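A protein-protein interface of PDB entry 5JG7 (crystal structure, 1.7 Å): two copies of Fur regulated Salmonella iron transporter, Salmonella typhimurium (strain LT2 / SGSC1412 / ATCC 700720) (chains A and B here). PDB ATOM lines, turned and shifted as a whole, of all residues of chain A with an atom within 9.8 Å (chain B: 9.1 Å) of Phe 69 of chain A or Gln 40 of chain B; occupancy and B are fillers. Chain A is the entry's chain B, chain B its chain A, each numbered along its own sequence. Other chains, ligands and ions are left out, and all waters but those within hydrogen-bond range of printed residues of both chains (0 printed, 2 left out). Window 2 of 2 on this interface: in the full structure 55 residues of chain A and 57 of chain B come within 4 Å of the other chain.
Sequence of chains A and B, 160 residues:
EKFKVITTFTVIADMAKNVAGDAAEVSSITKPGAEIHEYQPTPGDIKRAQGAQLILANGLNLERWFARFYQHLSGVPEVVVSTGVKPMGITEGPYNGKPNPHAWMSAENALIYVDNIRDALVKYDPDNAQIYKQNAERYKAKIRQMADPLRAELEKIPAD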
ATOM      1  N   LEU A  60       1.606  10.487  34.018  1.00  0.00           N
ATOM      2  CA  LEU A  60       0.698  10.637  32.890  1.00  0.00           C
ATOM      3  C   LEU A  60      -0.752  10.753  33.341  1.00  0.00           C
ATOM      4  O   LEU A  60      -1.546  11.460  32.708  1.00  0.00           O
ATOM      5  CB  LEU A  60       0.890   9.436  31.967  1.00  0.00           C
ATOM      6  CG  LEU A  60       0.435   9.386  30.526  1.00  0.00           C
ATOM      7  CD1 LEU A  60       0.927  10.621  29.764  1.00  0.00           C
ATOM      8  CD2 LEU A  60       0.992   8.097  29.924  1.00  0.00           C
ATOM      9  N   ASN A  61      -1.112  10.081  34.438  1.00  0.00           N
ATOM     10  CA  ASN A  61      -2.490  10.083  34.904  1.00  0.00           C
ATOM     11  C   ASN A  61      -2.965  11.463  35.330  1.00  0.00           C
ATOM     12  O   ASN A  61      -4.165  11.635  35.570  1.00  0.00           O
ATOM     13  CB  ASN A  61      -2.662   9.090  36.064  1.00  0.00           C
ATOM     14  CG  ASN A  61      -1.951   9.531  37.342  1.00  0.00           C
ATOM     15  OD1 ASN A  61      -0.958  10.268  37.312  1.00  0.00           O
ATOM     16  ND2 ASN A  61      -2.463   9.079  38.474  1.00  0.00           N
ATOM     17  N   GLU A  63      -2.044  14.277  33.380  1.00  0.00           N
ATOM     18  CA  GLU A  63      -2.140  15.095  32.179  1.00  0.00           C
ATOM     19  C   GLU A  63      -3.578  15.083  31.672  1.00  0.00           C
ATOM     20  O   GLU A  63      -4.177  14.016  31.520  1.00  0.00           O
ATOM     21  CB  GLU A  63      -1.179  14.588  31.102  1.00  0.00           C
ATOM     22  CG  GLU A  63       0.294  14.611  31.535  1.00  0.00           C
ATOM     23  CD  GLU A  63       1.256  14.221  30.421  1.00  0.00           C
ATOM     24  OE1 GLU A  63       0.923  14.405  29.228  1.00  0.00           O
ATOM     25  OE2 GLU A  63       2.354  13.727  30.740  1.00  0.00           O
ATOM     26  N   ARG A  64      -4.126  16.275  31.408  1.00  0.00           N
ATOM     27  CA  ARG A  64      -5.555  16.419  31.132  1.00  0.00           C
ATOM     28  C   ARG A  64      -6.028  15.473  30.035  1.00  0.00           C
ATOM     29  O   ARG A  64      -7.050  14.794  30.189  1.00  0.00           O
ATOM     30  CB  ARG A  64      -5.875  17.873  30.765  1.00  0.00           C
ATOM     31  N   TRP A  65      -5.291  15.401  28.922  1.00  0.00           N
ATOM     32  CA  TRP A  65      -5.723  14.569  27.802  1.00  0.00           C
ATOM     33  C   TRP A  65      -5.836  13.109  28.215  1.00  0.00           C
ATOM     34  O   TRP A  65      -6.729  12.387  27.752  1.00  0.00           O
ATOM     35  CB  TRP A  65      -4.748  14.714  26.635  1.00  0.00           C
ATOM     36  CG  TRP A  65      -3.403  14.085  26.887  1.00  0.00           C
ATOM     37  CD1 TRP A  65      -2.335  14.659  27.508  1.00  0.00           C
ATOM     38  CD2 TRP A  65      -2.993  12.764  26.523  1.00  0.00           C
ATOM     39  NE1 TRP A  65      -1.280  13.777  27.553  1.00  0.00           N
ATOM     40  CE2 TRP A  65      -1.662  12.604  26.957  1.00  0.00           C
ATOM     41  CE3 TRP A  65      -3.624  11.696  25.874  1.00  0.00           C
ATOM     42  CZ2 TRP A  65      -0.949  11.423  26.758  1.00  0.00           C
ATOM     43  CZ3 TRP A  65      -2.912  10.525  25.678  1.00  0.00           C
ATOM     44  CH2 TRP A  65      -1.587  10.399  26.120  1.00  0.00           C
ATOM     45  N   PHE A  66      -4.942  12.663  29.091  1.00  0.00           N
ATOM     46  CA  PHE A  66      -4.908  11.270  29.514  1.00  0.00           C
ATOM     47  C   PHE A  66      -5.926  11.014  30.616  1.00  0.00           C
ATOM     48  O   PHE A  66      -6.662  10.021  30.569  1.00  0.00           O
ATOM     49  CB  PHE A  66      -3.483  10.922  29.971  1.00  0.00           C
ATOM     50  CG  PHE A  66      -3.252   9.463  30.230  1.00  0.00           C
ATOM     51  CD1 PHE A  66      -2.864   8.612  29.209  1.00  0.00           C
ATOM     52  CD2 PHE A  66      -3.387   8.950  31.508  1.00  0.00           C
ATOM     53  CE1 PHE A  66      -2.633   7.275  29.462  1.00  0.00           C
ATOM     54  CE2 PHE A  66      -3.159   7.614  31.765  1.00  0.00           C
ATOM     55  CZ  PHE A  66      -2.782   6.779  30.747  1.00  0.00           C
ATOM     56  N   ALA A  67      -6.009  11.918  31.593  1.00  0.00           N
ATOM     57  CA  ALA A  67      -6.990  11.758  32.663  1.00  0.00           C
ATOM     58  C   ALA A  67      -8.422  11.801  32.138  1.00  0.00           C
ATOM     59  O   ALA A  67      -9.316  11.187  32.730  1.00  0.00           O
ATOM     60  CB  ALA A  67      -6.782  12.836  33.729  1.00  0.00           C
ATOM     61  N   ARG A  68      -8.670  12.510  31.036  1.00  0.00           N
ATOM     62  CA  ARG A  68     -10.042  12.590  30.534  1.00  0.00           C
ATOM     63  C   ARG A  68     -10.505  11.279  29.904  1.00  0.00           C
ATOM     64  O   ARG A  68     -11.697  10.956  29.970  1.00  0.00           O
ATOM     65  CB  ARG A  68     -10.180  13.736  29.529  1.00  0.00           C
ATOM     66  CG  ARG A  68     -10.231  15.110  30.172  1.00  0.00           C
ATOM     67  CD  ARG A  68     -10.331  16.235  29.143  1.00  0.00           C
ATOM     68  NE  ARG A  68     -11.616  16.243  28.448  1.00  0.00           N
ATOM     69  CZ  ARG A  68     -11.757  16.217  27.126  1.00  0.00           C
ATOM     70  NH1 ARG A  68     -10.687  16.190  26.341  1.00  0.00           N
ATOM     71  NH2 ARG A  68     -12.969  16.228  26.587  1.00  0.00           N
ATOM     72  N   PHE A  69      -9.597  10.500  29.311  1.00  0.00           N
ATOM     73  CA  PHE A  69     -10.001   9.347  28.515  1.00  0.00           C
ATOM     74  C   PHE A  69      -9.388   8.019  28.937  1.00  0.00           C
ATOM     75  O   PHE A  69      -9.786   6.976  28.397  1.00  0.00           O
ATOM     76  CB  PHE A  69      -9.666   9.582  27.038  1.00  0.00           C
ATOM     77  CG  PHE A  69     -10.448  10.696  26.413  1.00  0.00           C
ATOM     78  CD1 PHE A  69      -9.897  11.957  26.284  1.00  0.00           C
ATOM     79  CD2 PHE A  69     -11.739  10.482  25.958  1.00  0.00           C
ATOM     80  CE1 PHE A  69     -10.610  12.983  25.712  1.00  0.00           C
ATOM     81  CE2 PHE A  69     -12.460  11.505  25.383  1.00  0.00           C
ATOM     82  CZ  PHE A  69     -11.900  12.759  25.262  1.00  0.00           C
ATOM     83  N   TYR A  70      -8.432   8.014  29.850  1.00  0.00           N
ATOM     84  CA  TYR A  70      -7.825   6.785  30.337  1.00  0.00           C
ATOM     85  C   TYR A  70      -7.879   6.729  31.858  1.00  0.00           C
ATOM     86  O   TYR A  70      -6.900   6.365  32.520  1.00  0.00           O
ATOM     87  CB  TYR A  70      -6.381   6.658  29.876  1.00  0.00           C
ATOM     88  CG  TYR A  70      -6.139   6.681  28.388  1.00  0.00           C
ATOM     89  CD1 TYR A  70      -6.139   5.509  27.638  1.00  0.00           C
ATOM     90  CD2 TYR A  70      -5.845   7.866  27.741  1.00  0.00           C
ATOM     91  CE1 TYR A  70      -5.869   5.531  26.289  1.00  0.00           C
ATOM     92  CE2 TYR A  70      -5.582   7.892  26.387  1.00  0.00           C
ATOM     93  CZ  TYR A  70      -5.588   6.725  25.669  1.00  0.00           C
ATOM     94  OH  TYR A  70      -5.321   6.768  24.323  1.00  0.00           O
ATOM     95  N   GLN A  71      -9.022   7.100  32.438  1.00  0.00           N
ATOM     96  CA  GLN A  71      -9.146   7.095  33.898  1.00  0.00           C
ATOM     97  C   GLN A  71      -8.862   5.720  34.493  1.00  0.00           C
ATOM     98  O   GLN A  71      -8.323   5.624  35.602  1.00  0.00           O
ATOM     99  CB  GLN A  71     -10.544   7.558  34.322  1.00  0.00           C
ATOM    100  CG  GLN A  71     -10.973   8.875  33.720  1.00  0.00           C
ATOM    101  CD  GLN A  71     -12.258   9.421  34.325  1.00  0.00           C
ATOM    102  OE1 GLN A  71     -12.511   9.270  35.521  1.00  0.00           O
ATOM    103  NE2 GLN A  71     -13.078  10.059  33.491  1.00  0.00           N
ATOM    104  N   HIS A  72      -9.220   4.648  33.780  1.00  0.00           N
ATOM    105  CA  HIS A  72      -9.047   3.293  34.290  1.00  0.00           C
ATOM    106  C   HIS A  72      -7.587   2.925  34.529  1.00  0.00           C
ATOM    107  O   HIS A  72      -7.322   1.894  35.160  1.00  0.00           O
ATOM    108  CB  HIS A  72      -9.652   2.299  33.313  1.00  0.00           C
ATOM    109  CG  HIS A  72      -9.060   2.373  31.942  1.00  0.00           C
ATOM    110  ND1 HIS A  72      -9.266   3.448  31.101  1.00  0.00           N
ATOM    111  CD2 HIS A  72      -8.282   1.502  31.257  1.00  0.00           C
ATOM    112  CE1 HIS A  72      -8.629   3.237  29.962  1.00  0.00           C
ATOM    113  NE2 HIS A  72      -8.027   2.063  30.028  1.00  0.00           N
ATOM    114  N   LEU A  73      -6.645   3.714  34.020  1.00  0.00           N
ATOM    115  CA  LEU A  73      -5.222   3.468  34.199  1.00  0.00           C
ATOM    116  C   LEU A  73      -4.611   4.330  35.290  1.00  0.00           C
ATOM    117  O   LEU A  73      -3.383   4.375  35.409  1.00  0.00           O
ATOM    118  CB  LEU A  73      -4.480   3.709  32.884  1.00  0.00           C
ATOM    119  CG  LEU A  73      -4.956   2.880  31.694  1.00  0.00           C
ATOM    120  CD1 LEU A  73      -4.120   3.190  30.456  1.00  0.00           C
ATOM    121  CD2 LEU A  73      -4.894   1.398  32.018  1.00  0.00           C
ATOM    122  N   SER A  74      -5.442   5.002  36.093  1.00  0.00           N
ATOM    123  CA  SER A  74      -4.925   5.931  37.094  1.00  0.00           C
ATOM    124  C   SER A  74      -4.009   5.240  38.099  1.00  0.00           C
ATOM    125  O   SER A  74      -3.075   5.865  38.611  1.00  0.00           O
ATOM    126  CB  SER A  74      -6.083   6.622  37.814  1.00  0.00           C
ATOM    127  OG  SER A  74      -6.932   5.676  38.441  1.00  0.00           O
ATOM    128  N   ILE B  29       1.158   4.650  22.584  1.00  0.00           N
ATOM    129  CA  ILE B  29       0.018   5.505  22.297  1.00  0.00           C
ATOM    130  C   ILE B  29       0.562   6.899  22.032  1.00  0.00           C
ATOM    131  O   ILE B  29       1.699   7.219  22.385  1.00  0.00           O
ATOM    132  CB  ILE B  29      -1.017   5.516  23.438  1.00  0.00           C
ATOM    133  CG1 ILE B  29      -0.394   6.049  24.734  1.00  0.00           C
ATOM    134  CG2 ILE B  29      -1.614   4.082  23.653  1.00  0.00           C
ATOM    135  CD1 ILE B  29      -1.380   6.202  25.883  1.00  0.00           C
ATOM    136  N   THR B  30      -0.249   7.730  21.380  1.00  0.00           N
ATOM    137  CA  THR B  30       0.200   9.054  20.973  1.00  0.00           C
ATOM    138  C   THR B  30      -0.155  10.092  22.038  1.00  0.00           C
ATOM    139  O   THR B  30      -1.282  10.126  22.542  1.00  0.00           O
ATOM    140  CB  THR B  30      -0.409   9.427  19.616  1.00  0.00           C
ATOM    141  OG1 THR B  30       0.089   8.522  18.622  1.00  0.00           O
ATOM    142  CG2 THR B  30      -0.014  10.841  19.234  1.00  0.00           C
ATOM    143  N   PRO B  32      -0.334  14.190  22.695  1.00  0.00           N
ATOM    144  CA  PRO B  32      -0.325  15.452  21.945  1.00  0.00           C
ATOM    145  C   PRO B  32       0.788  16.376  22.421  1.00  0.00           C
ATOM    146  O   PRO B  32       1.212  16.338  23.577  1.00  0.00           O
ATOM    147  CB  PRO B  32      -1.706  16.047  22.238  1.00  0.00           C
ATOM    148  CG  PRO B  32      -2.049  15.508  23.587  1.00  0.00           C
ATOM    149  CD  PRO B  32      -1.475  14.107  23.626  1.00  0.00           C
ATOM    150  N   ILE B  36      -3.027  20.806  24.191  1.00  0.00           N
ATOM    151  CA  ILE B  36      -4.124  20.767  23.232  1.00  0.00           C
ATOM    152  C   ILE B  36      -5.463  20.751  23.961  1.00  0.00           C
ATOM    153  O   ILE B  36      -5.663  19.960  24.890  1.00  0.00           O
ATOM    154  CB  ILE B  36      -3.997  19.545  22.323  1.00  0.00           C
ATOM    155  N   HIS B  37      -6.380  21.623  23.527  1.00  0.00           N
ATOM    156  CA  HIS B  37      -7.663  21.773  24.209  1.00  0.00           C
ATOM    157  C   HIS B  37      -8.461  20.475  24.186  1.00  0.00           C
ATOM    158  O   HIS B  37      -8.742  19.881  25.233  1.00  0.00           O
ATOM    159  CB  HIS B  37      -8.465  22.909  23.570  1.00  0.00           C
ATOM    160  N   GLU B  38      -8.845  20.024  22.996  1.00  0.00           N
ATOM    161  CA  GLU B  38      -9.600  18.786  22.826  1.00  0.00           C
ATOM    162  C   GLU B  38      -8.730  17.811  22.039  1.00  0.00           C
ATOM    163  O   GLU B  38      -8.589  17.940  20.817  1.00  0.00           O
ATOM    164  CB  GLU B  38     -10.929  19.047  22.120  1.00  0.00           C
ATOM    165  N   TYR B  39      -8.130  16.842  22.732  1.00  0.00           N
ATOM    166  CA  TYR B  39      -7.381  15.776  22.069  1.00  0.00           C
ATOM    167  C   TYR B  39      -8.090  14.456  22.342  1.00  0.00           C
ATOM    168  O   TYR B  39      -7.944  13.872  23.419  1.00  0.00           O
ATOM    169  CB  TYR B  39      -5.929  15.715  22.523  1.00  0.00           C
ATOM    170  CG  TYR B  39      -5.164  14.660  21.759  1.00  0.00           C
ATOM    171  CD1 TYR B  39      -4.666  14.924  20.484  1.00  0.00           C
ATOM    172  CD2 TYR B  39      -4.972  13.391  22.289  1.00  0.00           C
ATOM    173  CE1 TYR B  39      -3.975  13.961  19.773  1.00  0.00           C
ATOM    174  CE2 TYR B  39      -4.285  12.421  21.584  1.00  0.00           C
ATOM    175  CZ  TYR B  39      -3.788  12.712  20.327  1.00  0.00           C
ATOM    176  OH  TYR B  39      -3.106  11.748  19.623  1.00  0.00           O
ATOM    177  N   GLN B  40      -8.824  13.989  21.356  1.00  0.00           N
ATOM    178  CA  GLN B  40      -9.589  12.758  21.473  1.00  0.00           C
ATOM    179  C   GLN B  40      -8.708  11.567  21.109  1.00  0.00           C
ATOM    180  O   GLN B  40      -8.011  11.610  20.094  1.00  0.00           O
ATOM    181  CB  GLN B  40     -10.804  12.811  20.552  1.00  0.00           C
ATOM    182  CG  GLN B  40     -11.697  11.593  20.625  1.00  0.00           C
ATOM    183  CD  GLN B  40     -12.981  11.872  21.365  1.00  0.00           C
ATOM    184  OE1 GLN B  40     -13.291  13.022  21.682  1.00  0.00           O
ATOM    185  NE2 GLN B  40     -13.742  10.823  21.643  1.00  0.00           N
ATOM    186  N   PRO B  41      -8.707  10.503  21.903  1.00  0.00           N
ATOM    187  CA  PRO B  41      -7.945   9.313  21.521  1.00  0.00           C
ATOM    188  C   PRO B  41      -8.540   8.650  20.298  1.00  0.00           C
ATOM    189  O   PRO B  41      -9.749   8.690  20.063  1.00  0.00           O
ATOM    190  CB  PRO B  41      -8.067   8.392  22.745  1.00  0.00           C
ATOM    191  CG  PRO B  41      -8.556   9.252  23.838  1.00  0.00           C
ATOM    192  CD  PRO B  41      -9.375  10.329  23.197  1.00  0.00           C
ATOM    193  N   THR B  42      -7.680   8.044  19.521  1.00  0.00           N
ATOM    194  CA  THR B  42      -8.188   7.192  18.469  1.00  0.00           C
ATOM    195  C   THR B  42      -8.673   5.873  19.060  1.00  0.00           C
ATOM    196  O   THR B  42      -8.242   5.471  20.144  1.00  0.00           O
ATOM    197  CB  THR B  42      -7.110   6.908  17.443  1.00  0.00           C
ATOM    198  OG1 THR B  42      -6.068   6.137  18.060  1.00  0.00           O
ATOM    199  CG2 THR B  42      -6.539   8.206  16.902  1.00  0.00           C
ATOM    200  N   PRO B  43      -9.573   5.179  18.366  1.00  0.00           N
ATOM    201  CA  PRO B  43      -9.931   3.823  18.810  1.00  0.00           C
ATOM    202  C   PRO B  43      -8.727   2.912  18.961  1.00  0.00           C
ATOM    203  O   PRO B  43      -8.673   2.114  19.906  1.00  0.00           O
ATOM    204  CB  PRO B  43     -10.881   3.345  17.704  1.00  0.00           C
ATOM    205  CG  PRO B  43     -11.492   4.597  17.185  1.00  0.00           C
ATOM    206  CD  PRO B  43     -10.408   5.633  17.239  1.00  0.00           C
ATOM    207  N   GLY B  44      -7.740   3.036  18.068  1.00  0.00           N
ATOM    208  CA  GLY B  44      -6.549   2.208  18.174  1.00  0.00           C
ATOM    209  C   GLY B  44      -5.783   2.437  19.467  1.00  0.00           C
ATOM    210  O   GLY B  44      -5.288   1.489  20.082  1.00  0.00           O
ATOM    211  N   ASP B  45      -5.672   3.698  19.896  1.00  0.00           N
ATOM    212  CA  ASP B  45      -4.970   3.964  21.153  1.00  0.00           C
ATOM    213  C   ASP B  45      -5.782   3.482  22.348  1.00  0.00           C
ATOM    214  O   ASP B  45      -5.217   2.996  23.335  1.00  0.00           O
ATOM    215  CB  ASP B  45      -4.653   5.454  21.297  1.00  0.00           C
ATOM    216  CG  ASP B  45      -3.364   5.862  20.588  1.00  0.00           C
ATOM    217  OD1 ASP B  45      -2.680   4.996  20.009  1.00  0.00           O
ATOM    218  OD2 ASP B  45      -3.029   7.066  20.622  1.00  0.00           O
ATOM    219  N   ILE B  46      -7.113   3.610  22.284  1.00  0.00           N
ATOM    220  CA  ILE B  46      -7.951   3.083  23.358  1.00  0.00           C
ATOM    221  C   ILE B  46      -7.706   1.590  23.532  1.00  0.00           C
ATOM    222  O   ILE B  46      -7.581   1.089  24.655  1.00  0.00           O
ATOM    223  CB  ILE B  46      -9.442   3.369  23.081  1.00  0.00           C
ATOM    224  CG1 ILE B  46      -9.748   4.869  23.133  1.00  0.00           C
ATOM    225  CG2 ILE B  46     -10.292   2.633  24.088  1.00  0.00           C
ATOM    226  CD1 ILE B  46      -9.546   5.502  24.492  1.00  0.00           C
ATOM    227  N   LYS B  47      -7.620   0.860  22.426  1.00  0.00           N
ATOM    228  CA  LYS B  47      -7.447  -0.583  22.533  1.00  0.00           C
ATOM    229  C   LYS B  47      -6.034  -0.934  22.976  1.00  0.00           C
ATOM    230  O   LYS B  47      -5.841  -1.868  23.761  1.00  0.00           O
ATOM    231  CB  LYS B  47      -7.780  -1.266  21.207  1.00  0.00           C
ATOM    232  CG  LYS B  47      -7.700  -2.781  21.293  1.00  0.00           C
ATOM    233  CD  LYS B  47      -8.011  -3.434  19.961  1.00  0.00           C
ATOM    234  CE  LYS B  47      -7.917  -4.949  20.060  1.00  0.00           C
ATOM    235  NZ  LYS B  47      -8.182  -5.601  18.746  1.00  0.00           N
ATOM    236  N   ALA B  49      -4.180   0.642  25.002  1.00  0.00           N
ATOM    237  CA  ALA B  49      -3.973   0.914  26.419  1.00  0.00           C
ATOM    238  C   ALA B  49      -4.740  -0.033  27.333  1.00  0.00           C
ATOM    239  O   ALA B  49      -4.489  -0.033  28.540  1.00  0.00           O
ATOM    240  CB  ALA B  49      -4.348   2.367  26.738  1.00  0.00           C
ATOM    241  N   GLN B  50      -5.649  -0.850  26.787  1.00  0.00           N
ATOM    242  CA  GLN B  50      -6.427  -1.781  27.600  1.00  0.00           C
ATOM    243  C   GLN B  50      -5.537  -2.721  28.400  1.00  0.00           C
ATOM    244  O   GLN B  50      -4.639  -3.364  27.852  1.00  0.00           O
ATOM    245  CB  GLN B  50      -7.353  -2.608  26.705  1.00  0.00           C
ATOM    246  CG  GLN B  50      -8.508  -1.829  26.187  1.00  0.00           C
ATOM    247  CD  GLN B  50      -9.359  -1.314  27.311  1.00  0.00           C
ATOM    248  OE1 GLN B  50      -9.816  -2.081  28.161  1.00  0.00           O
ATOM    249  NE2 GLN B  50      -9.560  -0.009  27.342  1.00  0.00           N
ATOM    250  N   PRO B  87      -8.139  12.293  39.144  1.00  0.00           N
ATOM    251  CA  PRO B  87      -8.186  13.760  39.138  1.00  0.00           C
ATOM    252  C   PRO B  87      -9.591  14.327  39.055  1.00  0.00           C
ATOM    253  O   PRO B  87      -9.937  15.013  38.089  1.00  0.00           O
ATOM    254  CB  PRO B  87      -7.365  14.133  37.895  1.00  0.00           C
ATOM    255  CG  PRO B  87      -6.619  12.881  37.514  1.00  0.00           C
ATOM    256  CD  PRO B  87      -7.513  11.759  37.929  1.00  0.00           C
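The backbone NH (N) of Thr 30 of chain B lies within hydrogen-bond range of the side-chain carboxylate (OD2) of Asp 45 of chain B, at 3.0 Å.
The backbone NH of Asp 45 of chain B sits at hydrogen-bond distance from the side-chain hydroxyl of Thr 42 of chain B, at 3.1 Å.
ND2 of Asn 61 of chain A is in hydrogen-bond range of O of Ser 74 of chain A (3.3 Å).
The indole nitrogen of Trp 65 of chain A sits at hydrogen-bond distance from the side-chain carboxylate of Glu 63 of chain A (2.8 Å).
CD2 of Trp 65 of chain A touches CD of Pro 32 of chain B, at 3.5 Å.
Phe 66 of chain A touches Ile 29 of chain B (CE1 to CD1, 3.9 Å).
CB of Ala 67 of chain A touches CG of Pro 87 of chain B (3.8 Å).
Phe 69 of chain A touches Tyr 39 of chain B (CE1 to O, 3.6 Å).
Phe 69 of chain A touches Gln 40 of chain B (CZ to OE1, 3.8 Å).
CB of Phe 69 of chain A touches CG of Pro 41 of chain B (3.4 Å).
Tyr 70 of chain A touches Pro 41 of chain B (OH to CB, 3.6 Å).
Tyr 70 of chain A touches Ala 49 of chain B (CE1 to CB, 3.5 Å).
His 72 of chain A touches Gln 50 of chain B (NE2 to NE2, 3.7 Å).
Leu 73 of chain A touches Ala 49 of chain B.
Of chain B, only Tyr 39 (3.6 Å), Gln 40 (3.8 Å) and Pro 41 (3.4 Å) come within 4 Å of Phe 69 of chain A.
Gln 40 of chain B touches just one residue of chain A: Phe 69.
Printed residues of chain A within 4 Å of Asp 45 of chain B: Tyr 70 (3.4 Å).
Of the printed residues of chain B, Leu 73 of chain A touches Ala 49.
Leu 60 of chain A touches none of the printed residues of chain B.
Lys 47 of chain B touches none of the printed residues of chain A.
The nearest residue of chain B that does not touch Phe 69 of chain A is Ile 46 of chain B (4.2 Å).
Of the 14 printed residues of chain A, 8 touch a printed residue of chain B.
Printed residues of chain A that touch a printed residue of chain B: Asn 61, Trp 65, Phe 66, Ala 67, Phe 69, Tyr 70, His 72 and Leu 73.
Hydrophobic or aromatic side chains of chain A within 4 Å of the printed part of chain B: Trp 65, Phe 66, Ala 67, Phe 69, Tyr 70, His 72 and Leu 73.
Among the printed residues, no Asp or Glu carboxylate lies within 4 Å of a Lys or Arg side-chain nitrogen of the other chain.
No position is printed for both chains.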
